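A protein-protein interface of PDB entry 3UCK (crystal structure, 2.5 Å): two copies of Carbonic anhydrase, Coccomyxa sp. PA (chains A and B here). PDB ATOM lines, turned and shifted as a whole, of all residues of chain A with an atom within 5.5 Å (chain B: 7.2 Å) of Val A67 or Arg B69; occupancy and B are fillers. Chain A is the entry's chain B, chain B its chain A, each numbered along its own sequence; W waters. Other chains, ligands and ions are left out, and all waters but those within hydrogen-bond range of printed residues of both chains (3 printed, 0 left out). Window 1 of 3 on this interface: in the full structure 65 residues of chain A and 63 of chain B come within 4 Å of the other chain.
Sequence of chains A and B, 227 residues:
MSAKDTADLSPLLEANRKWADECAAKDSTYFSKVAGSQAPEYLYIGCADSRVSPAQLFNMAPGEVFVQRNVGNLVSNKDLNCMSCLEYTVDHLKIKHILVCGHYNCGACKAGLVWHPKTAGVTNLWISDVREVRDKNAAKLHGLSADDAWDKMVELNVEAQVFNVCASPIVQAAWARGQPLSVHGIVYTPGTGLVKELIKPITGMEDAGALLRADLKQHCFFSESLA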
ATOM      1  N   LEU A  43      34.251   0.461 -11.750  1.00  0.00           N
ATOM      2  CA  LEU A  43      33.787  -0.492 -12.732  1.00  0.00           C
ATOM      3  C   LEU A  43      35.013  -1.314 -13.001  1.00  0.00           C
ATOM      4  O   LEU A  43      36.101  -0.713 -13.141  1.00  0.00           O
ATOM      5  CB  LEU A  43      33.389   0.221 -14.023  1.00  0.00           C
ATOM      6  CG  LEU A  43      33.301  -0.607 -15.308  1.00  0.00           C
ATOM      7  CD1 LEU A  43      32.230  -1.715 -15.248  1.00  0.00           C
ATOM      8  CD2 LEU A  43      33.130   0.341 -16.490  1.00  0.00           C
ATOM      9  N   TYR A  44      34.856  -2.643 -13.095  1.00  0.00           N
ATOM     10  CA  TYR A  44      35.940  -3.574 -13.435  1.00  0.00           C
ATOM     11  C   TYR A  44      35.619  -4.353 -14.686  1.00  0.00           C
ATOM     12  O   TYR A  44      34.510  -4.890 -14.843  1.00  0.00           O
ATOM     13  CB  TYR A  44      36.084  -4.583 -12.310  1.00  0.00           C
ATOM     14  CG  TYR A  44      36.977  -5.801 -12.553  1.00  0.00           C
ATOM     15  CD1 TYR A  44      38.312  -5.834 -12.095  1.00  0.00           C
ATOM     16  CD2 TYR A  44      36.465  -6.960 -13.158  1.00  0.00           C
ATOM     17  CE1 TYR A  44      39.121  -6.991 -12.277  1.00  0.00           C
ATOM     18  CE2 TYR A  44      37.252  -8.100 -13.337  1.00  0.00           C
ATOM     19  CZ  TYR A  44      38.571  -8.128 -12.891  1.00  0.00           C
ATOM     20  OH  TYR A  44      39.330  -9.240 -13.133  1.00  0.00           O
ATOM     21  N   PRO A  54      37.133 -10.358  -9.069  1.00  0.00           N
ATOM     22  CA  PRO A  54      37.559  -9.059  -8.575  1.00  0.00           C
ATOM     23  C   PRO A  54      37.120  -8.723  -7.160  1.00  0.00           C
ATOM     24  O   PRO A  54      37.956  -8.355  -6.352  1.00  0.00           O
ATOM     25  CB  PRO A  54      36.938  -8.086  -9.569  1.00  0.00           C
ATOM     26  CG  PRO A  54      35.888  -8.805 -10.188  1.00  0.00           C
ATOM     27  CD  PRO A  54      36.284 -10.212 -10.251  1.00  0.00           C
ATOM     28  N   ALA A  55      35.853  -8.850  -6.808  1.00  0.00           N
ATOM     29  CA  ALA A  55      35.504  -8.431  -5.450  1.00  0.00           C
ATOM     30  C   ALA A  55      36.311  -9.218  -4.418  1.00  0.00           C
ATOM     31  O   ALA A  55      36.680  -8.694  -3.345  1.00  0.00           O
ATOM     32  CB  ALA A  55      33.992  -8.540  -5.191  1.00  0.00           C
ATOM     33  N   VAL A  65      32.242  -2.860  -6.178  1.00  0.00           N
ATOM     34  CA  VAL A  65      32.680  -2.941  -7.603  1.00  0.00           C
ATOM     35  C   VAL A  65      31.657  -3.428  -8.641  1.00  0.00           C
ATOM     36  O   VAL A  65      31.138  -4.540  -8.542  1.00  0.00           O
ATOM     37  CB  VAL A  65      33.990  -3.778  -7.742  1.00  0.00           C
ATOM     38  CG1 VAL A  65      33.703  -5.255  -7.448  1.00  0.00           C
ATOM     39  CG2 VAL A  65      34.706  -3.554  -9.129  1.00  0.00           C
ATOM     40  N   PHE A  66      31.399  -2.618  -9.659  1.00  0.00           N
ATOM     41  CA  PHE A  66      30.544  -3.069 -10.744  1.00  0.00           C
ATOM     42  C   PHE A  66      31.421  -3.873 -11.717  1.00  0.00           C
ATOM     43  O   PHE A  66      32.550  -3.486 -12.018  1.00  0.00           O
ATOM     44  CB  PHE A  66      29.915  -1.874 -11.430  1.00  0.00           C
ATOM     45  CG  PHE A  66      28.527  -2.119 -11.995  1.00  0.00           C
ATOM     46  CD1 PHE A  66      27.384  -1.983 -11.182  1.00  0.00           C
ATOM     47  CD2 PHE A  66      28.355  -2.402 -13.346  1.00  0.00           C
ATOM     48  CE1 PHE A  66      26.126  -2.143 -11.686  1.00  0.00           C
ATOM     49  CE2 PHE A  66      27.084  -2.593 -13.879  1.00  0.00           C
ATOM     50  CZ  PHE A  66      25.972  -2.459 -13.053  1.00  0.00           C
ATOM     51  N   VAL A  67      30.901  -4.984 -12.215  1.00  0.00           N
ATOM     52  CA  VAL A  67      31.713  -5.984 -12.895  1.00  0.00           C
ATOM     53  C   VAL A  67      31.184  -6.326 -14.295  1.00  0.00           C
ATOM     54  O   VAL A  67      30.090  -6.850 -14.421  1.00  0.00           O
ATOM     55  CB  VAL A  67      31.796  -7.335 -12.044  1.00  0.00           C
ATOM     56  CG1 VAL A  67      32.450  -8.473 -12.858  1.00  0.00           C
ATOM     57  CG2 VAL A  67      32.560  -7.131 -10.766  1.00  0.00           C
ATOM     58  N   GLN A  68      31.960  -6.055 -15.343  1.00  0.00           N
ATOM     59  CA  GLN A  68      31.709  -6.695 -16.613  1.00  0.00           C
ATOM     60  C   GLN A  68      32.702  -7.873 -16.688  1.00  0.00           C
ATOM     61  O   GLN A  68      33.883  -7.692 -16.450  1.00  0.00           O
ATOM     62  CB  GLN A  68      31.936  -5.688 -17.725  1.00  0.00           C
ATOM     63  CG  GLN A  68      32.368  -6.234 -19.108  1.00  0.00           C
ATOM     64  CD  GLN A  68      31.295  -6.984 -19.896  1.00  0.00           C
ATOM     65  OE1 GLN A  68      31.587  -7.501 -20.971  1.00  0.00           O
ATOM     66  NE2 GLN A  68      30.058  -7.034 -19.393  1.00  0.00           N
ATOM     67  N   ARG A  69      32.267  -9.077 -16.997  1.00  0.00           N
ATOM     68  CA  ARG A  69      33.281 -10.154 -17.225  1.00  0.00           C
ATOM     69  C   ARG A  69      33.006 -10.889 -18.512  1.00  0.00           C
ATOM     70  O   ARG A  69      31.866 -11.249 -18.794  1.00  0.00           O
ATOM     71  CB  ARG A  69      33.386 -11.111 -16.038  1.00  0.00           C
ATOM     72  CG  ARG A  69      34.445 -10.639 -15.001  1.00  0.00           C
ATOM     73  CD  ARG A  69      34.400 -11.422 -13.716  1.00  0.00           C
ATOM     74  NE  ARG A  69      35.114 -12.699 -13.914  1.00  0.00           N
ATOM     75  CZ  ARG A  69      35.074 -13.716 -13.062  1.00  0.00           C
ATOM     76  NH1 ARG A  69      34.371 -13.624 -11.914  1.00  0.00           N
ATOM     77  NH2 ARG A  69      35.717 -14.845 -13.377  1.00  0.00           N
ATOM     78  N   ASN A  81      27.021  -5.229 -24.919  1.00  0.00           N
ATOM     79  CA  ASN A  81      27.038  -5.913 -23.630  1.00  0.00           C
ATOM     80  C   ASN A  81      27.936  -5.131 -22.693  1.00  0.00           C
ATOM     81  O   ASN A  81      27.491  -4.624 -21.662  1.00  0.00           O
ATOM     82  CB  ASN A  81      27.613  -7.335 -23.719  1.00  0.00           C
ATOM     83  CG  ASN A  81      27.541  -8.067 -22.394  1.00  0.00           C
ATOM     84  OD1 ASN A  81      27.070  -9.191 -22.340  1.00  0.00           O
ATOM     85  ND2 ASN A  81      27.908  -7.421 -21.323  1.00  0.00           N
ATOM     86  N   CYS A  85      27.470  -1.734 -19.547  1.00  0.00           N
ATOM     87  CA  CYS A  85      28.119  -1.698 -18.208  1.00  0.00           C
ATOM     88  C   CYS A  85      28.886  -0.390 -18.064  1.00  0.00           C
ATOM     89  O   CYS A  85      28.889   0.249 -17.009  1.00  0.00           O
ATOM     90  CB  CYS A  85      29.069  -2.883 -18.026  1.00  0.00           C
ATOM     91  SG  CYS A  85      28.236  -4.492 -17.673  1.00  0.00           S
ATOM     92  N   TYR B  44      28.516 -19.242 -14.275  1.00  0.00           N
ATOM     93  CA  TYR B  44      27.537 -18.371 -13.686  1.00  0.00           C
ATOM     94  C   TYR B  44      27.303 -17.207 -14.590  1.00  0.00           C
ATOM     95  O   TYR B  44      28.221 -16.579 -15.047  1.00  0.00           O
ATOM     96  CB  TYR B  44      28.008 -17.922 -12.314  1.00  0.00           C
ATOM     97  CG  TYR B  44      27.305 -16.768 -11.665  1.00  0.00           C
ATOM     98  CD1 TYR B  44      26.502 -16.953 -10.579  1.00  0.00           C
ATOM     99  CD2 TYR B  44      27.495 -15.490 -12.101  1.00  0.00           C
ATOM    100  CE1 TYR B  44      25.896 -15.908  -9.981  1.00  0.00           C
ATOM    101  CE2 TYR B  44      26.901 -14.450 -11.501  1.00  0.00           C
ATOM    102  CZ  TYR B  44      26.106 -14.655 -10.449  1.00  0.00           C
ATOM    103  OH  TYR B  44      25.516 -13.594  -9.886  1.00  0.00           O
ATOM    104  N   ILE B  45      26.033 -16.978 -14.871  1.00  0.00           N
ATOM    105  CA  ILE B  45      25.521 -15.842 -15.608  1.00  0.00           C
ATOM    106  C   ILE B  45      24.660 -15.005 -14.621  1.00  0.00           C
ATOM    107  O   ILE B  45      23.613 -15.459 -14.155  1.00  0.00           O
ATOM    108  CB  ILE B  45      24.680 -16.321 -16.803  1.00  0.00           C
ATOM    109  CG1 ILE B  45      25.505 -17.244 -17.716  1.00  0.00           C
ATOM    110  CG2 ILE B  45      24.182 -15.118 -17.631  1.00  0.00           C
ATOM    111  CD1 ILE B  45      24.700 -17.968 -18.742  1.00  0.00           C
ATOM    112  N   GLY B  46      25.106 -13.794 -14.308  1.00  0.00           N
ATOM    113  CA  GLY B  46      24.396 -12.926 -13.378  1.00  0.00           C
ATOM    114  C   GLY B  46      24.561 -11.468 -13.722  1.00  0.00           C
ATOM    115  O   GLY B  46      25.185 -11.135 -14.725  1.00  0.00           O
ATOM    116  N   CYS B  47      24.091 -10.583 -12.863  1.00  0.00           N
ATOM    117  CA  CYS B  47      24.037  -9.182 -13.203  1.00  0.00           C
ATOM    118  C   CYS B  47      25.333  -8.476 -12.898  1.00  0.00           C
ATOM    119  O   CYS B  47      26.052  -8.844 -11.944  1.00  0.00           O
ATOM    120  CB  CYS B  47      22.860  -8.491 -12.488  1.00  0.00           C
ATOM    121  SG  CYS B  47      22.646  -6.757 -12.994  1.00  0.00           S
ATOM    122  N   ALA B  48      25.644  -7.447 -13.684  1.00  0.00           N
ATOM    123  CA  ALA B  48      26.857  -6.648 -13.437  1.00  0.00           C
ATOM    124  C   ALA B  48      26.848  -5.872 -12.113  1.00  0.00           C
ATOM    125  O   ALA B  48      27.866  -5.304 -11.706  1.00  0.00           O
ATOM    126  CB  ALA B  48      27.133  -5.714 -14.569  1.00  0.00           C
ATOM    127  N   ASP B  49      25.698  -5.876 -11.440  1.00  0.00           N
ATOM    128  CA  ASP B  49      25.492  -5.184 -10.156  1.00  0.00           C
ATOM    129  C   ASP B  49      26.550  -5.413  -9.057  1.00  0.00           C
ATOM    130  O   ASP B  49      26.869  -6.552  -8.686  1.00  0.00           O
ATOM    131  CB  ASP B  49      24.094  -5.519  -9.603  1.00  0.00           C
ATOM    132  CG  ASP B  49      23.720  -4.666  -8.389  1.00  0.00           C
ATOM    133  OD1 ASP B  49      24.215  -4.962  -7.299  1.00  0.00           O
ATOM    134  OD2 ASP B  49      22.948  -3.707  -8.530  1.00  0.00           O
ATOM    135  N   SER B  50      27.026  -4.307  -8.492  1.00  0.00           N
ATOM    136  CA  SER B  50      28.096  -4.335  -7.487  1.00  0.00           C
ATOM    137  C   SER B  50      27.811  -5.095  -6.197  1.00  0.00           C
ATOM    138  O   SER B  50      28.778  -5.384  -5.433  1.00  0.00           O
ATOM    139  CB  SER B  50      28.550  -2.930  -7.109  1.00  0.00           C
ATOM    140  OG  SER B  50      27.531  -2.226  -6.415  1.00  0.00           O
ATOM    141  N   ARG B  51      26.540  -5.432  -5.936  1.00  0.00           N
ATOM    142  CA  ARG B  51      26.230  -6.169  -4.722  1.00  0.00           C
ATOM    143  C   ARG B  51      26.248  -7.686  -4.941  1.00  0.00           C
ATOM    144  O   ARG B  51      25.886  -8.469  -4.018  1.00  0.00           O
ATOM    145  CB  ARG B  51      24.896  -5.722  -4.158  1.00  0.00           C
ATOM    146  CG  ARG B  51      24.865  -4.230  -3.939  1.00  0.00           C
ATOM    147  CD  ARG B  51      23.462  -3.721  -3.860  1.00  0.00           C
ATOM    148  NE  ARG B  51      22.815  -3.519  -5.152  1.00  0.00           N
ATOM    149  CZ  ARG B  51      21.533  -3.186  -5.286  1.00  0.00           C
ATOM    150  NH1 ARG B  51      20.750  -3.036  -4.208  1.00  0.00           N
ATOM    151  NH2 ARG B  51      21.023  -3.014  -6.483  1.00  0.00           N
ATOM    152  N   VAL B  52      26.649  -8.123  -6.142  1.00  0.00           N
ATOM    153  CA  VAL B  52      26.427  -9.541  -6.451  1.00  0.00           C
ATOM    154  C   VAL B  52      27.657 -10.241  -6.999  1.00  0.00           C
ATOM    155  O   VAL B  52      27.875 -10.335  -8.245  1.00  0.00           O
ATOM    156  CB  VAL B  52      25.166  -9.769  -7.310  1.00  0.00           C
ATOM    157  CG1 VAL B  52      24.794 -11.254  -7.338  1.00  0.00           C
ATOM    158  CG2 VAL B  52      23.990  -8.901  -6.778  1.00  0.00           C
ATOM    159  N   SER B  53      28.465 -10.699  -6.046  1.00  0.00           N
ATOM    160  CA  SER B  53      29.769 -11.288  -6.305  1.00  0.00           C
ATOM    161  C   SER B  53      29.685 -12.816  -6.191  1.00  0.00           C
ATOM    162  O   SER B  53      29.694 -13.338  -5.090  1.00  0.00           O
ATOM    163  CB  SER B  53      30.740 -10.728  -5.287  1.00  0.00           C
ATOM    164  OG  SER B  53      32.066 -10.970  -5.675  1.00  0.00           O
ATOM    165  N   PRO B  54      29.554 -13.528  -7.321  1.00  0.00           N
ATOM    166  CA  PRO B  54      29.270 -14.957  -7.315  1.00  0.00           C
ATOM    167  C   PRO B  54      30.160 -15.732  -6.340  1.00  0.00           C
ATOM    168  O   PRO B  54      29.659 -16.459  -5.452  1.00  0.00           O
ATOM    169  CB  PRO B  54      29.587 -15.397  -8.730  1.00  0.00           C
ATOM    170  CG  PRO B  54      29.903 -14.140  -9.502  1.00  0.00           C
ATOM    171  CD  PRO B  54      29.641 -12.974  -8.673  1.00  0.00           C
ATOM    172  N   ALA B  55      31.462 -15.538  -6.482  1.00  0.00           N
ATOM    173  CA  ALA B  55      32.415 -16.256  -5.668  1.00  0.00           C
ATOM    174  C   ALA B  55      32.217 -15.968  -4.186  1.00  0.00           C
ATOM    175  O   ALA B  55      32.171 -16.891  -3.383  1.00  0.00           O
ATOM    176  CB  ALA B  55      33.814 -15.950  -6.096  1.00  0.00           C
ATOM    177  N   VAL B  67      32.676 -16.994 -15.003  1.00  0.00           N
ATOM    178  CA  VAL B  67      31.612 -16.009 -14.828  1.00  0.00           C
ATOM    179  C   VAL B  67      31.396 -15.060 -16.010  1.00  0.00           C
ATOM    180  O   VAL B  67      32.298 -14.363 -16.386  1.00  0.00           O
ATOM    181  CB  VAL B  67      31.888 -15.214 -13.572  1.00  0.00           C
ATOM    182  CG1 VAL B  67      31.038 -13.993 -13.543  1.00  0.00           C
ATOM    183  CG2 VAL B  67      31.664 -16.099 -12.341  1.00  0.00           C
ATOM    184  N   GLN B  68      30.185 -15.077 -16.583  1.00  0.00           N
ATOM    185  CA  GLN B  68      29.654 -13.973 -17.374  1.00  0.00           C
ATOM    186  C   GLN B  68      28.768 -13.009 -16.483  1.00  0.00           C
ATOM    187  O   GLN B  68      27.852 -13.487 -15.810  1.00  0.00           O
ATOM    188  CB  GLN B  68      28.866 -14.505 -18.566  1.00  0.00           C
ATOM    189  CG  GLN B  68      27.767 -13.558 -18.999  1.00  0.00           C
ATOM    190  CD  GLN B  68      28.240 -12.428 -19.930  1.00  0.00           C
ATOM    191  OE1 GLN B  68      27.407 -11.660 -20.433  1.00  0.00           O
ATOM    192  NE2 GLN B  68      29.556 -12.327 -20.168  1.00  0.00           N
ATOM    193  N   ARG B  69      29.070 -11.704 -16.453  1.00  0.00           N
ATOM    194  CA  ARG B  69      28.165 -10.716 -15.827  1.00  0.00           C
ATOM    195  C   ARG B  69      27.824  -9.530 -16.705  1.00  0.00           C
ATOM    196  O   ARG B  69      28.711  -8.848 -17.236  1.00  0.00           O
ATOM    197  CB  ARG B  69      28.698 -10.155 -14.502  1.00  0.00           C
ATOM    198  CG  ARG B  69      28.592 -11.120 -13.337  1.00  0.00           C
ATOM    199  CD  ARG B  69      29.450 -10.666 -12.150  1.00  0.00           C
ATOM    200  NE  ARG B  69      28.828  -9.569 -11.422  1.00  0.00           N
ATOM    201  CZ  ARG B  69      29.342  -9.030 -10.336  1.00  0.00           C
ATOM    202  NH1 ARG B  69      30.481  -9.507  -9.859  1.00  0.00           N
ATOM    203  NH2 ARG B  69      28.710  -8.045  -9.717  1.00  0.00           N
ATOM    204  N   ASN B  70      26.525  -9.294 -16.864  1.00  0.00           N
ATOM    205  CA  ASN B  70      26.054  -8.171 -17.672  1.00  0.00           C
ATOM    206  C   ASN B  70      24.850  -7.535 -17.006  1.00  0.00           C
ATOM    207  O   ASN B  70      24.285  -8.075 -15.999  1.00  0.00           O
ATOM    208  CB  ASN B  70      25.718  -8.613 -19.108  1.00  0.00           C
ATOM    209  CG  ASN B  70      24.540  -9.587 -19.165  1.00  0.00           C
ATOM    210  OD1 ASN B  70      23.390  -9.254 -18.796  1.00  0.00           O
ATOM    211  ND2 ASN B  70      24.811 -10.795 -19.634  1.00  0.00           N
ATOM    212  N   VAL B  71      24.478  -6.379 -17.541  1.00  0.00           N
ATOM    213  CA  VAL B  71      23.309  -5.632 -17.067  1.00  0.00           C
ATOM    214  C   VAL B  71      22.000  -6.388 -17.325  1.00  0.00           C
ATOM    215  O   VAL B  71      21.519  -6.407 -18.440  1.00  0.00           O
ATOM    216  CB  VAL B  71      23.242  -4.209 -17.701  1.00  0.00           C
ATOM    217  CG1 VAL B  71      21.943  -3.539 -17.340  1.00  0.00           C
ATOM    218  CG2 VAL B  71      24.418  -3.374 -17.259  1.00  0.00           C
ATOM    219  N   GLY B  72      21.436  -6.994 -16.280  1.00  0.00           N
ATOM    220  CA  GLY B  72      20.164  -7.697 -16.353  1.00  0.00           C
ATOM    221  C   GLY B  72      20.340  -9.208 -16.412  1.00  0.00           C
ATOM    222  O   GLY B  72      19.355  -9.953 -16.587  1.00  0.00           O
ATOM    223  N   ASN B  73      21.585  -9.686 -16.322  1.00  0.00           N
ATOM    224  CA  ASN B  73      21.809 -11.094 -16.555  1.00  0.00           C
ATOM    225  C   ASN B  73      21.035 -11.617 -17.734  1.00  0.00           C
ATOM    226  O   ASN B  73      20.267 -12.507 -17.592  1.00  0.00           O
ATOM    227  CB  ASN B  73      21.525 -11.968 -15.300  1.00  0.00           C
ATOM    228  CG  ASN B  73      20.181 -11.699 -14.664  1.00  0.00           C
ATOM    229  OD1 ASN B  73      20.077 -10.904 -13.740  1.00  0.00           O
ATOM    230  ND2 ASN B  73      19.143 -12.386 -15.138  1.00  0.00           N
ATOM    231  N   LEU B  74      21.251 -11.042 -18.917  1.00  0.00           N
ATOM    232  CA  LEU B  74      20.538 -11.457 -20.113  1.00  0.00           C
ATOM    233  C   LEU B  74      21.307 -12.498 -20.955  1.00  0.00           C
ATOM    234  O   LEU B  74      22.528 -12.433 -21.045  1.00  0.00           O
ATOM    235  CB  LEU B  74      20.335 -10.217 -20.961  1.00  0.00           C
ATOM    236  CG  LEU B  74      19.542  -9.056 -20.354  1.00  0.00           C
ATOM    237  CD1 LEU B  74      19.471  -7.880 -21.381  1.00  0.00           C
ATOM    238  CD2 LEU B  74      18.138  -9.470 -19.887  1.00  0.00           C
ATOM    239  N   ASN B  81      29.202 -11.920 -26.751  1.00  0.00           N
ATOM    240  CA  ASN B  81      29.851 -11.804 -25.460  1.00  0.00           C
ATOM    241  C   ASN B  81      29.386 -12.987 -24.571  1.00  0.00           C
ATOM    242  O   ASN B  81      30.185 -13.801 -24.157  1.00  0.00           O
ATOM    243  CB  ASN B  81      29.430 -10.475 -24.869  1.00  0.00           C
ATOM    244  CG  ASN B  81      30.201 -10.087 -23.625  1.00  0.00           C
ATOM    245  OD1 ASN B  81      30.354 -10.879 -22.691  1.00  0.00           O
ATOM    246  ND2 ASN B  81      30.625  -8.806 -23.577  1.00  0.00           N
ATOM    247  N   CYS B  85      31.276 -17.027 -23.481  1.00  0.00           N
ATOM    248  CA  CYS B  85      31.389 -17.625 -22.168  1.00  0.00           C
ATOM    249  C   CYS B  85      30.648 -18.937 -22.169  1.00  0.00           C
ATOM    250  O   CYS B  85      31.117 -19.903 -21.590  1.00  0.00           O
ATOM    251  CB  CYS B  85      30.791 -16.705 -21.122  1.00  0.00           C
ATOM    252  SG  CYS B  85      31.627 -15.094 -20.993  1.00  0.00           S
HETATM  253  O   HOH W   1      25.766  -5.346 -19.798  1.00  0.00           O
HETATM  254  O   HOH W   2      31.701  -4.824  -4.820  1.00  0.00           O
HETATM  255  O   HOH W   3      33.784 -10.692  -7.686  1.00  0.00           O
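The side-chain amide oxygen (OE1) of Gln B68 lies close to the side-chain amide oxygen (OD1) of Asn A81, at 3.1 Å. O of Arg B69 lies within hydrogen-bond range of NE2 of Gln A68 (3.1 Å). OE1 of Gln A68 is in hydrogen-bond range of ND2 of Asn B81 (3.1 Å). The backbone carbonyl oxygen (O) of Ala B48 is in hydrogen-bond range of the backbone NH (N) of Val A67, at 3.1 Å. The side-chain amide nitrogen (NE2) of Gln B68 sits at hydrogen-bond distance from the backbone carbonyl oxygen (O) of Arg A69, at 2.9 Å.
The side-chain amide nitrogen (NE2) of Gln B68 lies within hydrogen-bond range of the side-chain amide oxygen (OD1) of Asn B81, at 3.0 Å. NH2 of Arg B69 lies within hydrogen-bond range of O of Ala B48 (3.5 Å). NE2 of Gln A68 is in hydrogen-bond range of SG of Cys A85. The side-chain sulfur of Cys B47 sits close to the backbone NH of Asp B49, 3.5 Å away. O of Tyr B44 is in hydrogen-bond range of N of Gln B68, at 2.9 Å. O of Asn B81 lies within hydrogen-bond range of SG of Cys B85, 3.7 Å away.
CB of Ala A55 touches OG of Ser B53, 3.1 Å away. CE1 of Phe A66 touches CA of Asp B49 (3.5 Å). CD1 of Phe A66 touches N of Ser B50 (3.6 Å). CG2 of Val A67 touches NH1 of Arg B69, at 3.3 Å. Arg A69 touches Val B67. N of Arg A69 touches O of Arg B69, at 3.6 Å. Asn A81 touches Asn B70 (ND2 to CB, 3.3 Å). Asn B81 touches Asn A81 (ND2 to CB, 3.4 Å). SG of Cys A85 touches CB of Ala B48 (3.5 Å). Val B71 touches Cys A85.
Of the printed residues of chain B, Val A67 touches Ala B48 and Arg B69. Of chain A, only Val A67 (3.3 Å), Gln A68 (3.1 Å) and Arg A69 (3.6 Å) come within 4 Å of Arg B69. Printed residues of chain B within 4 Å of Asn A81: Gln B68 (3.1 Å), Asn B70 (3.3 Å) and Asn B81 (3.4 Å). Of the printed residues of chain B, Val A65 touches Ser B50. Of the printed residues of chain A, Gln B68 touches Arg A69 (2.9 Å) and Asn A81 (3.1 Å). Leu B74 touches none of the printed residues of chain A. Cys B47 touches none of the printed residues of chain A. The nearest printed residue of chain A that does not touch Arg B69 is Asn A81 (4.4 Å).
Of the 22 printed residues of chain B, 10 touch a printed residue of chain A. Printed residues of chain B that touch a printed residue of chain A: Ala B48, Asp B49, Ser B50, Ser B53, Val B67, Gln B68, Arg B69, Asn B70, Val B71 and Asn B81. Hydrophobic or aromatic side chains of chain A within 4 Å of the printed part of chain B: Ala A55, Phe A66 and Val A67. Along chain A the printed residues that touch a printed residue of chain B span positions 55 to 85. Among the printed residues, 17 pairs touch across the chains.
Gln A68 touches Arg B69, and with the chains exchanged Arg A69 touches Gln B68. Gln A68 touches Asn B81, and with the chains exchanged Asn A81 touches Gln B68. Arg A69 touches its own counterpart, Arg B69. Asn B81 touches its own counterpart, Asn A81. Positions printed for both chains: 44, 54, 55, 67, 68, 69, 81 and 85. Of the 17 pairs that touch across the chains among the printed residues, 8 have their exchanged pair printed and touching as well.
Water W2 bridges N of Val A65 (2.4 Å) and O of Ser B50 (3.0 Å). Water W1 lies within hydrogen-bond range of the backbone carbonyl oxygen of Asn A81, the backbone NH of Val B71 and the side-chain sulfur of Cys A85. Water W3 lies within hydrogen-bond range of the side-chain hydroxyl (OG) of Ser B53 and the backbone NH (N) of Ala A55.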
